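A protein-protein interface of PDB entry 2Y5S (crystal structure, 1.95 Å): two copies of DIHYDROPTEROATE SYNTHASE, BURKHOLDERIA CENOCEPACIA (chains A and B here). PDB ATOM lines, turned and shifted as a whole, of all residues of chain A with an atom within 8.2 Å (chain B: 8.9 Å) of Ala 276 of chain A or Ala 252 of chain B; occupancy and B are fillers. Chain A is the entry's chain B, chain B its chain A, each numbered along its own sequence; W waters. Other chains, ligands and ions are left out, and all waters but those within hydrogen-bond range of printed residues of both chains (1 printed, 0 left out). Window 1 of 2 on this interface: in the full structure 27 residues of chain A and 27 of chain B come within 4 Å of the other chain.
Ala 252 of chain A touches Ala 276 of chain B, and with the chains exchanged Ala 276 of chain A touches Ala 252 of chain B.
Ala 256 of chain A touches Leu 259 of chain B, and with the chains exchanged Leu 259 of chain A touches Ala 256 of chain B.
Ala 256 of chain A touches Ala 280 of chain B, and with the chains exchanged Ala 280 of chain A touches Ala 256 of chain B.
Leu 259 of chain B touches its own counterpart, Leu 259 of chain A.
11 positions are printed for both chains.
O of Lys 245 of chain B lies within hydrogen-bond range of NE of Arg 250 of chain B, 2.9 Å away.
The side-chain carboxylate of Asp 279 of chain A is in salt-bridge range of the side-chain amino group of Lys 245 of chain B (2.7 Å).
Of the 22 printed residues of chain A, 7 touch a printed residue of chain B.
Hydrophobic or aromatic side chains of chain A within 4 Å of the printed part of chain B: Ala 252, Ala 256, Leu 259, Ala 276, Ala 280 and Val 283.
Of the 21 printed residues of chain B, 9 touch a printed residue of chain A.
Hydrophobic or aromatic side chains of chain B within 4 Å of the printed part of chain A: Ile 242, Ala 252, Ala 253, Ala 256, Leu 259, Ala 276 and Ala 280.
O of Ala 276 of chain B touches CB of Ala 252 of chain A (3.3 Å).
Leu 259 of chain B touches Ala 256 of chain A (CD1 to CB, 3.6 Å).
Ala 256 of chain A touches Ala 280 of chain B (CB to CA, 3.6 Å).
Ala 256 of chain B touches Leu 259 of chain A.
Ala 252 of chain B touches Ala 276 of chain A.
Ile 242 of chain B touches Asp 279 of chain A.
CB of Ala 256 of chain B touches O of Ala 280 of chain A (3.6 Å).
Val 283 of chain A touches Ala 253 of chain B.
Ala 256 of chain B touches Val 283 of chain A.
Val 283 of chain A touches Ala 257 of chain B (CG1 to N, 3.98 Å).
Ala 276 of chain A touches one residue of chain B.
Of chain A, only Ala 276 comes within 4 Å of Ala 252 of chain B.
No residue of chain B comes within 4 Å of Ala 275 of chain A.
Ala 253 of chain B touches just one residue of chain A: Val 283.
Of the printed residues of chain B, Ala 256 of chain A touches Leu 259 and Ala 280.
Printed residues of chain A within 4 Å of Ile 242 of chain B: Asp 279 (3.5 Å).
Printed residues of chain A within 4 Å of Lys 245 of chain B: Asp 279 (2.7 Å).
Of the printed residues of chain A, Leu 259 of chain B touches Ala 256 and Leu 259.
Arg 250 of chain B touches none of the printed residues of chain A.
Thr 277 of chain A touches none of the printed residues of chain B.
The nearest residue of chain B that does not touch Ala 276 of chain A is Ala 253 of chain B (5.4 Å).
The nearest printed residue of chain A that does not touch Ala 252 of chain B is Asp 279 of chain A (4.3 Å).
Water W1 lies within hydrogen-bond range of the side-chain carboxylate (OD2) of Asp 279 of chain A (2.9 Å), the backbone NH (N) of Ala 253 of chain B (3.1 Å), the backbone carbonyl oxygen (O) of Glu 249 of chain B (3.1 Å) and the backbone NH (N) of Ala 252 of chain B (3.3 Å).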
ATOM      1  N   VAL A  25     -26.496 -12.549  -5.411  1.00  0.00           N
ATOM      2  CA  VAL A  25     -25.820 -11.313  -5.064  1.00  0.00           C
ATOM      3  C   VAL A  25     -25.112 -10.689  -6.305  1.00  0.00           C
ATOM      4  O   VAL A  25     -24.246 -11.302  -6.950  1.00  0.00           O
ATOM      5  CB  VAL A  25     -24.841 -11.578  -3.930  1.00  0.00           C
ATOM      6  CG1 VAL A  25     -24.006 -10.341  -3.628  1.00  0.00           C
ATOM      7  CG2 VAL A  25     -25.633 -12.093  -2.689  1.00  0.00           C
ATOM      8  N   GLU A  58     -15.412 -13.387  -3.116  1.00  0.00           N
ATOM      9  CA  GLU A  58     -16.266 -13.148  -1.946  1.00  0.00           C
ATOM     10  C   GLU A  58     -17.672 -13.749  -2.091  1.00  0.00           C
ATOM     11  O   GLU A  58     -18.429 -13.752  -1.142  1.00  0.00           O
ATOM     12  CB  GLU A  58     -16.377 -11.649  -1.642  1.00  0.00           C
ATOM     13  CG  GLU A  58     -15.112 -11.057  -1.045  1.00  0.00           C
ATOM     14  CD  GLU A  58     -15.193  -9.554  -0.865  1.00  0.00           C
ATOM     15  OE1 GLU A  58     -16.296  -8.979  -0.956  1.00  0.00           O
ATOM     16  OE2 GLU A  58     -14.148  -8.933  -0.616  1.00  0.00           O
ATOM     17  N   VAL A 251     -22.606   0.003   6.074  1.00  0.00           N
ATOM     18  CA  VAL A 251     -22.497  -1.398   5.669  1.00  0.00           C
ATOM     19  C   VAL A 251     -23.511  -2.263   6.407  1.00  0.00           C
ATOM     20  O   VAL A 251     -24.241  -3.027   5.764  1.00  0.00           O
ATOM     21  CB  VAL A 251     -21.067  -1.970   5.853  1.00  0.00           C
ATOM     22  CG1 VAL A 251     -21.008  -3.431   5.385  1.00  0.00           C
ATOM     23  CG2 VAL A 251     -20.029  -1.100   5.108  1.00  0.00           C
ATOM     24  N   ALA A 252     -23.565  -2.157   7.738  1.00  0.00           N
ATOM     25  CA  ALA A 252     -24.521  -2.970   8.506  1.00  0.00           C
ATOM     26  C   ALA A 252     -25.953  -2.664   8.129  1.00  0.00           C
ATOM     27  O   ALA A 252     -26.773  -3.572   7.990  1.00  0.00           O
ATOM     28  CB  ALA A 252     -24.317  -2.814  10.024  1.00  0.00           C
ATOM     29  N   SER A 254     -26.915  -1.646   5.224  1.00  0.00           N
ATOM     30  CA  SER A 254     -27.070  -2.198   3.858  1.00  0.00           C
ATOM     31  C   SER A 254     -27.313  -3.703   3.901  1.00  0.00           C
ATOM     32  O   SER A 254     -28.204  -4.226   3.233  1.00  0.00           O
ATOM     33  CB  SER A 254     -25.832  -1.894   3.002  1.00  0.00           C
ATOM     34  OG  SER A 254     -25.596  -0.506   2.863  1.00  0.00           O
ATOM     35  N   VAL A 255     -26.555  -4.400   4.738  1.00  0.00           N
ATOM     36  CA  VAL A 255     -26.826  -5.816   4.984  1.00  0.00           C
ATOM     37  C   VAL A 255     -28.265  -6.022   5.490  1.00  0.00           C
ATOM     38  O   VAL A 255     -28.973  -6.911   4.997  1.00  0.00           O
ATOM     39  CB  VAL A 255     -25.786  -6.394   5.975  1.00  0.00           C
ATOM     40  CG1 VAL A 255     -26.148  -7.808   6.399  1.00  0.00           C
ATOM     41  CG2 VAL A 255     -24.403  -6.367   5.331  1.00  0.00           C
ATOM     42  N   ALA A 256     -28.701  -5.210   6.455  1.00  0.00           N
ATOM     43  CA  ALA A 256     -30.071  -5.317   6.992  1.00  0.00           C
ATOM     44  C   ALA A 256     -31.112  -5.151   5.886  1.00  0.00           C
ATOM     45  O   ALA A 256     -32.082  -5.926   5.795  1.00  0.00           O
ATOM     46  CB  ALA A 256     -30.301  -4.287   8.135  1.00  0.00           C
ATOM     47  N   ALA A 258     -30.703  -5.571   2.535  1.00  0.00           N
ATOM     48  CA  ALA A 258     -30.626  -6.738   1.631  1.00  0.00           C
ATOM     49  C   ALA A 258     -31.350  -7.953   2.193  1.00  0.00           C
ATOM     50  O   ALA A 258     -32.133  -8.607   1.487  1.00  0.00           O
ATOM     51  CB  ALA A 258     -29.157  -7.058   1.296  1.00  0.00           C
ATOM     52  N   LEU A 259     -31.148  -8.232   3.487  1.00  0.00           N
ATOM     53  CA  LEU A 259     -31.889  -9.321   4.153  1.00  0.00           C
ATOM     54  C   LEU A 259     -33.385  -9.142   4.150  1.00  0.00           C
ATOM     55  O   LEU A 259     -34.145 -10.092   3.906  1.00  0.00           O
ATOM     56  CB  LEU A 259     -31.429  -9.479   5.605  1.00  0.00           C
ATOM     57  CG  LEU A 259     -30.078 -10.162   5.800  1.00  0.00           C
ATOM     58  CD1 LEU A 259     -29.519  -9.883   7.208  1.00  0.00           C
ATOM     59  CD2 LEU A 259     -30.198 -11.692   5.516  1.00  0.00           C
ATOM     60  N   VAL A 271     -25.292  -4.945  -4.445  1.00  0.00           N
ATOM     61  CA  VAL A 271     -24.576  -4.479  -3.265  1.00  0.00           C
ATOM     62  C   VAL A 271     -23.129  -4.099  -3.534  1.00  0.00           C
ATOM     63  O   VAL A 271     -22.498  -4.577  -4.496  1.00  0.00           O
ATOM     64  CB  VAL A 271     -24.612  -5.558  -2.166  1.00  0.00           C
ATOM     65  CG1 VAL A 271     -26.065  -5.993  -1.887  1.00  0.00           C
ATOM     66  CG2 VAL A 271     -23.748  -6.787  -2.573  1.00  0.00           C
ATOM     67  N   HIS A 272     -22.612  -3.238  -2.667  1.00  0.00           N
ATOM     68  CA  HIS A 272     -21.195  -2.900  -2.653  1.00  0.00           C
ATOM     69  C   HIS A 272     -20.426  -3.913  -1.831  1.00  0.00           C
ATOM     70  O   HIS A 272     -19.330  -4.311  -2.199  1.00  0.00           O
ATOM     71  CB  HIS A 272     -20.989  -1.526  -2.024  1.00  0.00           C
ATOM     72  CG  HIS A 272     -21.553  -0.404  -2.833  1.00  0.00           C
ATOM     73  ND1 HIS A 272     -22.797   0.134  -2.590  1.00  0.00           N
ATOM     74  CD2 HIS A 272     -21.034   0.288  -3.878  1.00  0.00           C
ATOM     75  CE1 HIS A 272     -23.024   1.107  -3.458  1.00  0.00           C
ATOM     76  NE2 HIS A 272     -21.968   1.223  -4.246  1.00  0.00           N
ATOM     77  N   ASP A 273     -21.018  -4.323  -0.710  1.00  0.00           N
ATOM     78  CA  ASP A 273     -20.306  -5.116   0.296  1.00  0.00           C
ATOM     79  C   ASP A 273     -20.631  -6.590   0.134  1.00  0.00           C
ATOM     80  O   ASP A 273     -21.534  -7.112   0.777  1.00  0.00           O
ATOM     81  CB  ASP A 273     -20.645  -4.591   1.688  1.00  0.00           C
ATOM     82  CG  ASP A 273     -20.387  -3.127   1.807  1.00  0.00           C
ATOM     83  OD1 ASP A 273     -19.197  -2.779   1.937  1.00  0.00           O
ATOM     84  OD2 ASP A 273     -21.352  -2.320   1.698  1.00  0.00           O
ATOM     85  N   VAL A 274     -19.890  -7.253  -0.744  1.00  0.00           N
ATOM     86  CA  VAL A 274     -20.276  -8.575  -1.205  1.00  0.00           C
ATOM     87  C   VAL A 274     -20.087  -9.646  -0.123  1.00  0.00           C
ATOM     88  O   VAL A 274     -21.016 -10.395   0.155  1.00  0.00           O
ATOM     89  CB  VAL A 274     -19.505  -8.975  -2.471  1.00  0.00           C
ATOM     90  CG1 VAL A 274     -19.818 -10.440  -2.847  1.00  0.00           C
ATOM     91  CG2 VAL A 274     -19.857  -8.012  -3.598  1.00  0.00           C
ATOM     92  N   ALA A 275     -18.899  -9.707   0.484  1.00  0.00           N
ATOM     93  CA  ALA A 275     -18.625 -10.709   1.525  1.00  0.00           C
ATOM     94  C   ALA A 275     -19.650 -10.634   2.652  1.00  0.00           C
ATOM     95  O   ALA A 275     -20.128 -11.677   3.150  1.00  0.00           O
ATOM     96  CB  ALA A 275     -17.195 -10.547   2.111  1.00  0.00           C
ATOM     97  N   ALA A 276     -19.927  -9.412   3.104  1.00  0.00           N
ATOM     98  CA  ALA A 276     -20.847  -9.209   4.207  1.00  0.00           C
ATOM     99  C   ALA A 276     -22.257  -9.635   3.839  1.00  0.00           C
ATOM    100  O   ALA A 276     -22.960 -10.238   4.650  1.00  0.00           O
ATOM    101  CB  ALA A 276     -20.825  -7.726   4.682  1.00  0.00           C
ATOM    102  N   THR A 277     -22.678  -9.323   2.618  1.00  0.00           N
ATOM    103  CA  THR A 277     -24.002  -9.716   2.145  1.00  0.00           C
ATOM    104  C   THR A 277     -24.122 -11.230   2.016  1.00  0.00           C
ATOM    105  O   THR A 277     -25.113 -11.825   2.443  1.00  0.00           O
ATOM    106  CB  THR A 277     -24.348  -9.003   0.811  1.00  0.00           C
ATOM    107  OG1 THR A 277     -24.207  -7.587   0.989  1.00  0.00           O
ATOM    108  CG2 THR A 277     -25.770  -9.275   0.388  1.00  0.00           C
ATOM    109  N   VAL A 278     -23.099 -11.843   1.445  1.00  0.00           N
ATOM    110  CA  VAL A 278     -23.056 -13.281   1.270  1.00  0.00           C
ATOM    111  C   VAL A 278     -23.107 -14.027   2.611  1.00  0.00           C
ATOM    112  O   VAL A 278     -23.891 -14.966   2.776  1.00  0.00           O
ATOM    113  CB  VAL A 278     -21.817 -13.681   0.444  1.00  0.00           C
ATOM    114  CG1 VAL A 278     -21.573 -15.196   0.514  1.00  0.00           C
ATOM    115  CG2 VAL A 278     -21.981 -13.191  -1.057  1.00  0.00           C
ATOM    116  N   ASP A 279     -22.293 -13.594   3.562  1.00  0.00           N
ATOM    117  CA  ASP A 279     -22.299 -14.156   4.923  1.00  0.00           C
ATOM    118  C   ASP A 279     -23.693 -14.045   5.551  1.00  0.00           C
ATOM    119  O   ASP A 279     -24.213 -15.030   6.121  1.00  0.00           O
ATOM    120  CB  ASP A 279     -21.258 -13.461   5.809  1.00  0.00           C
ATOM    121  CG  ASP A 279     -19.820 -13.932   5.548  1.00  0.00           C
ATOM    122  OD1 ASP A 279     -19.601 -14.923   4.809  1.00  0.00           O
ATOM    123  OD2 ASP A 279     -18.886 -13.309   6.117  1.00  0.00           O
ATOM    124  N   ALA A 280     -24.300 -12.858   5.449  1.00  0.00           N
ATOM    125  CA  ALA A 280     -25.656 -12.646   5.948  1.00  0.00           C
ATOM    126  C   ALA A 280     -26.631 -13.583   5.288  1.00  0.00           C
ATOM    127  O   ALA A 280     -27.470 -14.153   5.958  1.00  0.00           O
ATOM    128  CB  ALA A 280     -26.116 -11.186   5.769  1.00  0.00           C
ATOM    129  N   LEU A 281     -26.496 -13.776   3.976  1.00  0.00           N
ATOM    130  CA  LEU A 281     -27.415 -14.652   3.248  1.00  0.00           C
ATOM    131  C   LEU A 281     -27.147 -16.138   3.542  1.00  0.00           C
ATOM    132  O   LEU A 281     -28.039 -16.959   3.395  1.00  0.00           O
ATOM    133  CB  LEU A 281     -27.390 -14.350   1.727  1.00  0.00           C
ATOM    134  CG  LEU A 281     -28.086 -13.045   1.290  1.00  0.00           C
ATOM    135  CD1 LEU A 281     -27.994 -12.845  -0.219  1.00  0.00           C
ATOM    136  CD2 LEU A 281     -29.557 -12.990   1.722  1.00  0.00           C
ATOM    137  N   SER A 282     -25.941 -16.492   3.963  1.00  0.00           N
ATOM    138  CA  SER A 282     -25.685 -17.862   4.413  1.00  0.00           C
ATOM    139  C   SER A 282     -26.484 -18.163   5.696  1.00  0.00           C
ATOM    140  O   SER A 282     -27.090 -19.234   5.841  1.00  0.00           O
ATOM    141  CB  SER A 282     -24.194 -18.111   4.663  1.00  0.00           C
ATOM    142  OG  SER A 282     -23.437 -18.041   3.477  1.00  0.00           O
ATOM    143  N   VAL A 283     -26.504 -17.199   6.611  1.00  0.00           N
ATOM    144  CA  VAL A 283     -27.283 -17.343   7.828  1.00  0.00           C
ATOM    145  C   VAL A 283     -28.772 -17.420   7.487  1.00  0.00           C
ATOM    146  O   VAL A 283     -29.478 -18.284   7.976  1.00  0.00           O
ATOM    147  CB  VAL A 283     -26.998 -16.197   8.808  1.00  0.00           C
ATOM    148  CG1 VAL A 283     -27.988 -16.254  10.016  1.00  0.00           C
ATOM    149  CG2 VAL A 283     -25.519 -16.247   9.265  1.00  0.00           C
ATOM    150  N   ARG B 234     -21.137 -13.892  17.077  1.00  0.00           N
ATOM    151  CA  ARG B 234     -19.823 -14.486  16.788  1.00  0.00           C
ATOM    152  C   ARG B 234     -19.693 -15.982  17.096  1.00  0.00           C
ATOM    153  O   ARG B 234     -18.590 -16.516  17.146  1.00  0.00           O
ATOM    154  CB  ARG B 234     -18.718 -13.710  17.512  1.00  0.00           C
ATOM    155  CG  ARG B 234     -18.626 -12.265  17.065  1.00  0.00           C
ATOM    156  CD  ARG B 234     -17.495 -11.533  17.779  1.00  0.00           C
ATOM    157  NE  ARG B 234     -17.358 -10.141  17.303  1.00  0.00           N
ATOM    158  CZ  ARG B 234     -16.481  -9.266  17.805  1.00  0.00           C
ATOM    159  NH1 ARG B 234     -15.652  -9.618  18.794  1.00  0.00           N
ATOM    160  NH2 ARG B 234     -16.429  -8.022  17.328  1.00  0.00           N
ATOM    161  N   LEU B 238     -22.602 -19.642  13.463  1.00  0.00           N
ATOM    162  CA  LEU B 238     -22.393 -18.693  12.372  1.00  0.00           C
ATOM    163  C   LEU B 238     -21.187 -19.097  11.549  1.00  0.00           C
ATOM    164  O   LEU B 238     -21.257 -19.123  10.321  1.00  0.00           O
ATOM    165  CB  LEU B 238     -22.218 -17.273  12.910  1.00  0.00           C
ATOM    166  CG  LEU B 238     -23.266 -16.714  13.844  1.00  0.00           C
ATOM    167  CD1 LEU B 238     -22.975 -15.218  14.218  1.00  0.00           C
ATOM    168  CD2 LEU B 238     -24.663 -16.872  13.227  1.00  0.00           C
ATOM    169  N   ILE B 242     -20.621 -20.046   7.155  1.00  0.00           N
ATOM    170  CA  ILE B 242     -19.889 -19.073   6.337  1.00  0.00           C
ATOM    171  C   ILE B 242     -18.480 -19.568   5.989  1.00  0.00           C
ATOM    172  O   ILE B 242     -17.564 -18.773   5.771  1.00  0.00           O
ATOM    173  CB  ILE B 242     -19.879 -17.623   6.982  1.00  0.00           C
ATOM    174  CG1 ILE B 242     -19.054 -17.556   8.267  1.00  0.00           C
ATOM    175  CG2 ILE B 242     -21.295 -17.148   7.269  1.00  0.00           C
ATOM    176  CD1 ILE B 242     -19.163 -16.180   8.999  1.00  0.00           C
ATOM    177  N   LYS B 245     -15.017 -19.326   8.974  1.00  0.00           N
ATOM    178  CA  LYS B 245     -14.310 -18.113   9.376  1.00  0.00           C
ATOM    179  C   LYS B 245     -14.262 -17.984  10.913  1.00  0.00           C
ATOM    180  O   LYS B 245     -15.206 -18.395  11.609  1.00  0.00           O
ATOM    181  CB  LYS B 245     -14.998 -16.873   8.810  1.00  0.00           C
ATOM    182  CG  LYS B 245     -14.957 -16.702   7.294  1.00  0.00           C
ATOM    183  CD  LYS B 245     -15.813 -15.474   6.952  1.00  0.00           C
ATOM    184  CE  LYS B 245     -15.857 -15.162   5.480  1.00  0.00           C
ATOM    185  NZ  LYS B 245     -16.383 -13.782   5.297  1.00  0.00           N
ATOM    186  N   PRO B 247     -13.974 -16.065  14.853  1.00  0.00           N
ATOM    187  CA  PRO B 247     -14.912 -15.178  15.555  1.00  0.00           C
ATOM    188  C   PRO B 247     -14.931 -13.719  15.105  1.00  0.00           C
ATOM    189  O   PRO B 247     -16.015 -13.168  14.860  1.00  0.00           O
ATOM    190  CB  PRO B 247     -14.464 -15.293  17.006  1.00  0.00           C
ATOM    191  CG  PRO B 247     -13.988 -16.692  17.117  1.00  0.00           C
ATOM    192  CD  PRO B 247     -13.286 -16.967  15.805  1.00  0.00           C
ATOM    193  N   LEU B 248     -13.763 -13.102  14.958  1.00  0.00           N
ATOM    194  CA  LEU B 248     -13.694 -11.690  14.575  1.00  0.00           C
ATOM    195  C   LEU B 248     -14.167 -11.424  13.146  1.00  0.00           C
ATOM    196  O   LEU B 248     -14.345 -10.265  12.774  1.00  0.00           O
ATOM    197  CB  LEU B 248     -12.261 -11.140  14.740  1.00  0.00           C
ATOM    198  CG  LEU B 248     -11.663 -11.241  16.145  1.00  0.00           C
ATOM    199  CD1 LEU B 248     -10.158 -10.861  16.134  1.00  0.00           C
ATOM    200  CD2 LEU B 248     -12.453 -10.366  17.117  1.00  0.00           C
ATOM    201  N   GLU B 249     -14.380 -12.479  12.348  1.00  0.00           N
ATOM    202  CA  GLU B 249     -14.814 -12.330  10.956  1.00  0.00           C
ATOM    203  C   GLU B 249     -16.279 -12.759  10.763  1.00  0.00           C
ATOM    204  O   GLU B 249     -16.712 -13.060   9.645  1.00  0.00           O
ATOM    205  CB  GLU B 249     -13.894 -13.127  10.027  1.00  0.00           C
ATOM    206  CG  GLU B 249     -12.425 -12.650  10.068  1.00  0.00           C
ATOM    207  CD  GLU B 249     -11.484 -13.490   9.208  1.00  0.00           C
ATOM    208  OE1 GLU B 249     -11.950 -14.125   8.240  1.00  0.00           O
ATOM    209  OE2 GLU B 249     -10.258 -13.503   9.499  1.00  0.00           O
ATOM    210  N   ARG B 250     -17.041 -12.752  11.852  1.00  0.00           N
ATOM    211  CA  ARG B 250     -18.419 -13.210  11.849  1.00  0.00           C
ATOM    212  C   ARG B 250     -19.373 -12.042  12.101  1.00  0.00           C
ATOM    213  O   ARG B 250     -20.528 -12.266  12.500  1.00  0.00           O
ATOM    214  CB  ARG B 250     -18.625 -14.294  12.929  1.00  0.00           C
ATOM    215  CG  ARG B 250     -17.900 -15.624  12.661  1.00  0.00           C
ATOM    216  CD  ARG B 250     -18.052 -16.624  13.818  1.00  0.00           C
ATOM    217  NE  ARG B 250     -17.109 -17.719  13.641  1.00  0.00           N
ATOM    218  CZ  ARG B 250     -16.756 -18.623  14.554  1.00  0.00           C
ATOM    219  NH1 ARG B 250     -17.260 -18.619  15.777  1.00  0.00           N
ATOM    220  NH2 ARG B 250     -15.847 -19.537  14.228  1.00  0.00           N
ATOM    221  N   VAL B 251     -18.925 -10.800  11.892  1.00  0.00           N
ATOM    222  CA  VAL B 251     -19.787  -9.659  12.254  1.00  0.00           C
ATOM    223  C   VAL B 251     -21.046  -9.601  11.369  1.00  0.00           C
ATOM    224  O   VAL B 251     -22.154  -9.468  11.886  1.00  0.00           O
ATOM    225  CB  VAL B 251     -19.071  -8.296  12.224  1.00  0.00           C
ATOM    226  CG1 VAL B 251     -20.057  -7.192  12.609  1.00  0.00           C
ATOM    227  CG2 VAL B 251     -17.839  -8.282  13.170  1.00  0.00           C
ATOM    228  N   ALA B 252     -20.892  -9.696  10.043  1.00  0.00           N
ATOM    229  CA  ALA B 252     -22.064  -9.635   9.162  1.00  0.00           C
ATOM    230  C   ALA B 252     -23.036 -10.777   9.490  1.00  0.00           C
ATOM    231  O   ALA B 252     -24.244 -10.576   9.554  1.00  0.00           O
ATOM    232  CB  ALA B 252     -21.655  -9.665   7.685  1.00  0.00           C
ATOM    233  N   ALA B 253     -22.505 -11.963   9.751  1.00  0.00           N
ATOM    234  CA  ALA B 253     -23.344 -13.118  10.055  1.00  0.00           C
ATOM    235  C   ALA B 253     -24.059 -12.909  11.380  1.00  0.00           C
ATOM    236  O   ALA B 253     -25.232 -13.307  11.549  1.00  0.00           O
ATOM    237  CB  ALA B 253     -22.483 -14.406  10.088  1.00  0.00           C
ATOM    238  N   SER B 254     -23.363 -12.274  12.328  1.00  0.00           N
ATOM    239  CA  SER B 254     -23.965 -11.960  13.640  1.00  0.00           C
ATOM    240  C   SER B 254     -25.109 -10.970  13.516  1.00  0.00           C
ATOM    241  O   SER B 254     -26.137 -11.118  14.169  1.00  0.00           O
ATOM    242  CB  SER B 254     -22.925 -11.400  14.620  1.00  0.00           C
ATOM    243  OG  SER B 254     -21.874 -12.325  14.892  1.00  0.00           O
ATOM    244  N   VAL B 255     -24.952  -9.964  12.672  1.00  0.00           N
ATOM    245  CA  VAL B 255     -26.038  -9.015  12.411  1.00  0.00           C
ATOM    246  C   VAL B 255     -27.245  -9.735  11.818  1.00  0.00           C
ATOM    247  O   VAL B 255     -28.393  -9.437  12.203  1.00  0.00           O
ATOM    248  CB  VAL B 255     -25.586  -7.857  11.457  1.00  0.00           C
ATOM    249  CG1 VAL B 255     -26.784  -7.071  10.903  1.00  0.00           C
ATOM    250  CG2 VAL B 255     -24.589  -6.922  12.162  1.00  0.00           C
ATOM    251  N   ALA B 256     -27.005 -10.655  10.871  1.00  0.00           N
ATOM    252  CA  ALA B 256     -28.097 -11.387  10.215  1.00  0.00           C
ATOM    253  C   ALA B 256     -28.867 -12.225  11.229  1.00  0.00           C
ATOM    254  O   ALA B 256     -30.095 -12.299  11.185  1.00  0.00           O
ATOM    255  CB  ALA B 256     -27.586 -12.296   9.086  1.00  0.00           C
ATOM    256  N   ALA B 257     -28.132 -12.877  12.115  1.00  0.00           N
ATOM    257  CA  ALA B 257     -28.736 -13.692  13.165  1.00  0.00           C
ATOM    258  C   ALA B 257     -29.601 -12.844  14.119  1.00  0.00           C
ATOM    259  O   ALA B 257     -30.701 -13.232  14.458  1.00  0.00           O
ATOM    260  CB  ALA B 257     -27.632 -14.435  13.946  1.00  0.00           C
ATOM    261  N   ALA B 258     -29.093 -11.688  14.528  1.00  0.00           N
ATOM    262  CA  ALA B 258     -29.831 -10.779  15.422  1.00  0.00           C
ATOM    263  C   ALA B 258     -31.116 -10.304  14.752  1.00  0.00           C
ATOM    264  O   ALA B 258     -32.159 -10.272  15.373  1.00  0.00           O
ATOM    265  CB  ALA B 258     -28.948  -9.573  15.818  1.00  0.00           C
ATOM    266  N   LEU B 259     -31.034  -9.940  13.473  1.00  0.00           N
ATOM    267  CA  LEU B 259     -32.199  -9.493  12.728  1.00  0.00           C
ATOM    268  C   LEU B 259     -33.243 -10.592  12.612  1.00  0.00           C
ATOM    269  O   LEU B 259     -34.430 -10.335  12.776  1.00  0.00           O
ATOM    270  CB  LEU B 259     -31.794  -9.002  11.336  1.00  0.00           C
ATOM    271  CG  LEU B 259     -31.206  -7.607  11.232  1.00  0.00           C
ATOM    272  CD1 LEU B 259     -30.590  -7.406   9.836  1.00  0.00           C
ATOM    273  CD2 LEU B 259     -32.286  -6.523  11.546  1.00  0.00           C
ATOM    274  N   ASP B 273     -21.067  -6.542  18.703  1.00  0.00           N
ATOM    275  CA  ASP B 273     -20.954  -5.457  17.744  1.00  0.00           C
ATOM    276  C   ASP B 273     -22.152  -4.529  17.843  1.00  0.00           C
ATOM    277  O   ASP B 273     -23.153  -4.677  17.130  1.00  0.00           O
ATOM    278  CB  ASP B 273     -20.778  -6.055  16.347  1.00  0.00           C
ATOM    279  CG  ASP B 273     -19.611  -7.022  16.293  1.00  0.00           C
ATOM    280  OD1 ASP B 273     -18.485  -6.542  16.255  1.00  0.00           O
ATOM    281  OD2 ASP B 273     -19.809  -8.261  16.331  1.00  0.00           O
ATOM    282  N   ALA B 276     -23.096  -1.837  14.767  1.00  0.00           N
ATOM    283  CA  ALA B 276     -23.595  -2.585  13.619  1.00  0.00           C
ATOM    284  C   ALA B 276     -25.005  -3.143  13.858  1.00  0.00           C
ATOM    285  O   ALA B 276     -25.852  -3.096  12.958  1.00  0.00           O
ATOM    286  CB  ALA B 276     -22.627  -3.730  13.263  1.00  0.00           C
ATOM    287  N   THR B 277     -25.248  -3.712  15.047  1.00  0.00           N
ATOM    288  CA  THR B 277     -26.554  -4.281  15.378  1.00  0.00           C
ATOM    289  C   THR B 277     -27.642  -3.220  15.494  1.00  0.00           C
ATOM    290  O   THR B 277     -28.782  -3.450  15.058  1.00  0.00           O
ATOM    291  CB  THR B 277     -26.495  -5.098  16.723  1.00  0.00           C
ATOM    292  OG1 THR B 277     -25.468  -6.103  16.622  1.00  0.00           O
ATOM    293  CG2 THR B 277     -27.809  -5.760  17.004  1.00  0.00           C
ATOM    294  N   ALA B 280     -28.616  -2.021  12.041  1.00  0.00           N
ATOM    295  CA  ALA B 280     -29.452  -3.016  11.382  1.00  0.00           C
ATOM    296  C   ALA B 280     -30.874  -2.936  11.911  1.00  0.00           C
ATOM    297  O   ALA B 280     -31.826  -2.979  11.128  1.00  0.00           O
ATOM    298  CB  ALA B 280     -28.896  -4.430  11.586  1.00  0.00           C
HETATM  299  O   HOH W   1     -19.657 -12.541   8.819  1.00  0.00           O
